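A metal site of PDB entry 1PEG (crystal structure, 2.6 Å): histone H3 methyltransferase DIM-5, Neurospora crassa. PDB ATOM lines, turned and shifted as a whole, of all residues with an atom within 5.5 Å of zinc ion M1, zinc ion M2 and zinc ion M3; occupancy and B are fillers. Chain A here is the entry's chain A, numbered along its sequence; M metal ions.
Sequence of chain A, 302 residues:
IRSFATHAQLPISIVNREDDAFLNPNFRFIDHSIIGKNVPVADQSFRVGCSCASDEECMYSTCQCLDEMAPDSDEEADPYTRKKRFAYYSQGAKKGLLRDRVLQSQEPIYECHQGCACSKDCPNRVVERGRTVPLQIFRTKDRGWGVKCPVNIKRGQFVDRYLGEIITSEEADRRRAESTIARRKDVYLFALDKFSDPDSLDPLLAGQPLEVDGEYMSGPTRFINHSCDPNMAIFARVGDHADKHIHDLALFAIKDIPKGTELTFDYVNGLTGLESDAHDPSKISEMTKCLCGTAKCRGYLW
The backbone NH (N) of Cys 65 lies close to the side-chain sulfur (SG) of Cys 63 (3.7 Å). The side-chain sulfur (SG) of Cys 122 sits close to the backbone NH (N) of Asn 124, 3.4 Å away. The backbone NH (N) of Cys 112 is in hydrogen-bond range of the backbone carbonyl oxygen (O) of Asn 124 (2.8 Å). SG of Cys 116 lies close to N of His 113, at 3.6 Å.
Four residues have an atom within 4 Å of zinc ion M1: Cys 50, Cys 65, Cys 112 and Cys 116. The nearest printed residue that does not touch zinc ion M1 is Cys 63 (4.1 Å).
The nearest printed residue that does not touch zinc ion M2 is Cys 116 (4.6 Å).
Within 4 Å of zinc ion M3: Cys 50, Cys 52, Cys 58 and Cys 63. Along chain A the residues within 4 Å of zinc ion M3 span positions 50 to 63.
Zinc ion M1 is bound by SG of Cys 65 (2.3 Å), SG of Cys 50 (2.3 Å), SG of Cys 116 (2.3 Å) and SG of Cys 112 (2.4 Å). Zinc ion M1 has four donor atoms within binding distance.
Zinc ion M2 is bound by the side-chain sulfur (SG) of Cys 58, the side-chain sulfur (SG) of Cys 118, the side-chain sulfur (SG) of Cys 122 and the side-chain sulfur (SG) of Cys 112.
Zinc ion M3 is bound by SG of Cys 50 (2.3 Å), SG of Cys 58 (2.3 Å), SG of Cys 63 (2.3 Å) and SG of Cys 52 (2.3 Å). Zinc ion M3 has four donor atoms within binding distance.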
ATOM      1  N   GLY A  49      19.086  24.249   3.178  1.00  0.00           N
ATOM      2  CA  GLY A  49      20.017  23.204   3.503  1.00  0.00           C
ATOM      3  C   GLY A  49      19.222  21.944   3.339  1.00  0.00           C
ATOM      4  O   GLY A  49      18.171  21.949   2.712  1.00  0.00           O
ATOM      5  N   CYS A  50      19.707  20.844   3.907  1.00  0.00           N
ATOM      6  CA  CYS A  50      18.989  19.576   3.840  1.00  0.00           C
ATOM      7  C   CYS A  50      18.436  19.117   5.203  1.00  0.00           C
ATOM      8  O   CYS A  50      19.104  19.188   6.230  1.00  0.00           O
ATOM      9  CB  CYS A  50      19.864  18.485   3.182  1.00  0.00           C
ATOM     10  SG  CYS A  50      21.377  17.987   4.061  1.00  0.00           S
ATOM     11  N   CYS A  52      17.679  16.195   5.954  1.00  0.00           N
ATOM     12  CA  CYS A  52      18.183  14.871   6.234  1.00  0.00           C
ATOM     13  C   CYS A  52      18.206  14.687   7.743  1.00  0.00           C
ATOM     14  O   CYS A  52      18.444  15.625   8.506  1.00  0.00           O
ATOM     15  CB  CYS A  52      19.619  14.713   5.702  1.00  0.00           C
ATOM     16  SG  CYS A  52      19.774  14.430   3.913  1.00  0.00           S
ATOM     17  N   GLU A  57      22.878  11.140   6.105  1.00  0.00           N
ATOM     18  CA  GLU A  57      22.762  10.206   5.012  1.00  0.00           C
ATOM     19  C   GLU A  57      22.654  11.085   3.832  1.00  0.00           C
ATOM     20  O   GLU A  57      21.728  11.048   3.032  1.00  0.00           O
ATOM     21  CB  GLU A  57      21.550   9.286   5.145  1.00  0.00           C
ATOM     22  N   CYS A  58      23.715  11.907   3.740  1.00  0.00           N
ATOM     23  CA  CYS A  58      23.816  12.918   2.716  1.00  0.00           C
ATOM     24  C   CYS A  58      24.730  12.416   1.614  1.00  0.00           C
ATOM     25  O   CYS A  58      25.404  13.209   0.958  1.00  0.00           O
ATOM     26  CB  CYS A  58      24.382  14.235   3.296  1.00  0.00           C
ATOM     27  SG  CYS A  58      23.412  15.064   4.607  1.00  0.00           S
ATOM     28  N   CYS A  63      18.972  13.577  -0.716  1.00  0.00           N
ATOM     29  CA  CYS A  63      19.391  14.894  -0.165  1.00  0.00           C
ATOM     30  C   CYS A  63      19.303  15.975  -1.253  1.00  0.00           C
ATOM     31  O   CYS A  63      19.835  15.809  -2.355  1.00  0.00           O
ATOM     32  CB  CYS A  63      20.828  14.755   0.384  1.00  0.00           C
ATOM     33  SG  CYS A  63      21.621  16.218   1.147  1.00  0.00           S
ATOM     34  N   GLN A  64      18.626  17.080  -0.938  1.00  0.00           N
ATOM     35  CA  GLN A  64      18.437  18.187  -1.884  1.00  0.00           C
ATOM     36  C   GLN A  64      19.705  18.972  -2.204  1.00  0.00           C
ATOM     37  O   GLN A  64      19.688  19.851  -3.063  1.00  0.00           O
ATOM     38  CB  GLN A  64      17.365  19.153  -1.356  1.00  0.00           C
ATOM     39  N   CYS A  65      20.796  18.649  -1.516  1.00  0.00           N
ATOM     40  CA  CYS A  65      22.081  19.324  -1.722  1.00  0.00           C
ATOM     41  C   CYS A  65      22.729  18.893  -3.038  1.00  0.00           C
ATOM     42  O   CYS A  65      23.516  19.630  -3.632  1.00  0.00           O
ATOM     43  CB  CYS A  65      22.995  19.029  -0.519  1.00  0.00           C
ATOM     44  SG  CYS A  65      22.467  19.905   0.996  1.00  0.00           S
ATOM     45  N   GLU A 111      28.505  20.427  -1.596  1.00  0.00           N
ATOM     46  CA  GLU A 111      28.703  20.057  -0.198  1.00  0.00           C
ATOM     47  C   GLU A 111      27.603  20.617   0.681  1.00  0.00           C
ATOM     48  O   GLU A 111      26.867  21.517   0.279  1.00  0.00           O
ATOM     49  CB  GLU A 111      30.041  20.589   0.274  1.00  0.00           C
ATOM     50  CG  GLU A 111      31.030  19.555   0.738  1.00  0.00           C
ATOM     51  CD  GLU A 111      32.284  20.206   1.294  1.00  0.00           C
ATOM     52  OE1 GLU A 111      32.764  19.814   2.377  1.00  0.00           O
ATOM     53  OE2 GLU A 111      32.773  21.133   0.642  1.00  0.00           O
ATOM     54  N   CYS A 112      27.496  20.065   1.892  1.00  0.00           N
ATOM     55  CA  CYS A 112      26.505  20.514   2.852  1.00  0.00           C
ATOM     56  C   CYS A 112      27.042  21.774   3.559  1.00  0.00           C
ATOM     57  O   CYS A 112      28.147  22.222   3.245  1.00  0.00           O
ATOM     58  CB  CYS A 112      26.211  19.400   3.866  1.00  0.00           C
ATOM     59  SG  CYS A 112      24.921  18.230   3.321  1.00  0.00           S
ATOM     60  N   HIS A 113      26.267  22.336   4.483  1.00  0.00           N
ATOM     61  CA  HIS A 113      26.660  23.557   5.195  1.00  0.00           C
ATOM     62  C   HIS A 113      25.876  23.777   6.499  1.00  0.00           C
ATOM     63  O   HIS A 113      25.398  22.824   7.106  1.00  0.00           O
ATOM     64  CB  HIS A 113      26.457  24.764   4.290  1.00  0.00           C
ATOM     65  CG  HIS A 113      25.181  24.713   3.532  1.00  0.00           C
ATOM     66  ND1 HIS A 113      25.117  24.468   2.178  1.00  0.00           N
ATOM     67  CD2 HIS A 113      23.896  24.820   3.947  1.00  0.00           C
ATOM     68  CE1 HIS A 113      23.860  24.433   1.793  1.00  0.00           C
ATOM     69  NE2 HIS A 113      23.096  24.647   2.849  1.00  0.00           N
ATOM     70  N   CYS A 116      21.803  22.566   6.892  1.00  0.00           N
ATOM     71  CA  CYS A 116      21.268  21.226   6.835  1.00  0.00           C
ATOM     72  C   CYS A 116      21.142  20.545   8.191  1.00  0.00           C
ATOM     73  O   CYS A 116      21.879  20.858   9.131  1.00  0.00           O
ATOM     74  CB  CYS A 116      22.148  20.388   5.922  1.00  0.00           C
ATOM     75  SG  CYS A 116      22.855  21.331   4.554  1.00  0.00           S
ATOM     76  N   CYS A 118      22.231  18.025   9.392  1.00  0.00           N
ATOM     77  CA  CYS A 118      23.321  17.070   9.497  1.00  0.00           C
ATOM     78  C   CYS A 118      24.482  17.793  10.187  1.00  0.00           C
ATOM     79  O   CYS A 118      24.545  19.028  10.167  1.00  0.00           O
ATOM     80  CB  CYS A 118      23.720  16.571   8.105  1.00  0.00           C
ATOM     81  SG  CYS A 118      24.523  17.815   7.055  1.00  0.00           S
ATOM     82  N   CYS A 122      29.150  15.048   8.615  1.00  0.00           N
ATOM     83  CA  CYS A 122      28.400  14.782   7.401  1.00  0.00           C
ATOM     84  C   CYS A 122      29.408  14.524   6.280  1.00  0.00           C
ATOM     85  O   CYS A 122      30.158  15.413   5.859  1.00  0.00           O
ATOM     86  CB  CYS A 122      27.498  15.947   6.995  1.00  0.00           C
ATOM     87  SG  CYS A 122      26.915  15.785   5.264  1.00  0.00           S
ATOM     88  N   ASN A 124      29.549  14.639   3.357  1.00  0.00           N
ATOM     89  CA  ASN A 124      29.591  15.558   2.226  1.00  0.00           C
ATOM     90  C   ASN A 124      29.872  16.964   2.675  1.00  0.00           C
ATOM     91  O   ASN A 124      29.308  17.907   2.150  1.00  0.00           O
ATOM     92  CB  ASN A 124      28.261  15.525   1.503  1.00  0.00           C
ATOM     93  CG  ASN A 124      28.325  16.156   0.134  1.00  0.00           C
ATOM     94  OD1 ASN A 124      29.394  16.533  -0.319  1.00  0.00           O
ATOM     95  ND2 ASN A 124      27.179  16.267  -0.530  1.00  0.00           N
HETATM   96 ZN    ZN M   1      22.897  19.475   3.199  1.00  0.00          ZN
HETATM   97 ZN    ZN M   2      24.835  16.733   5.063  1.00  0.00          ZN
HETATM   98 ZN    ZN M   3      21.602  15.807   3.411  1.00  0.00          ZN
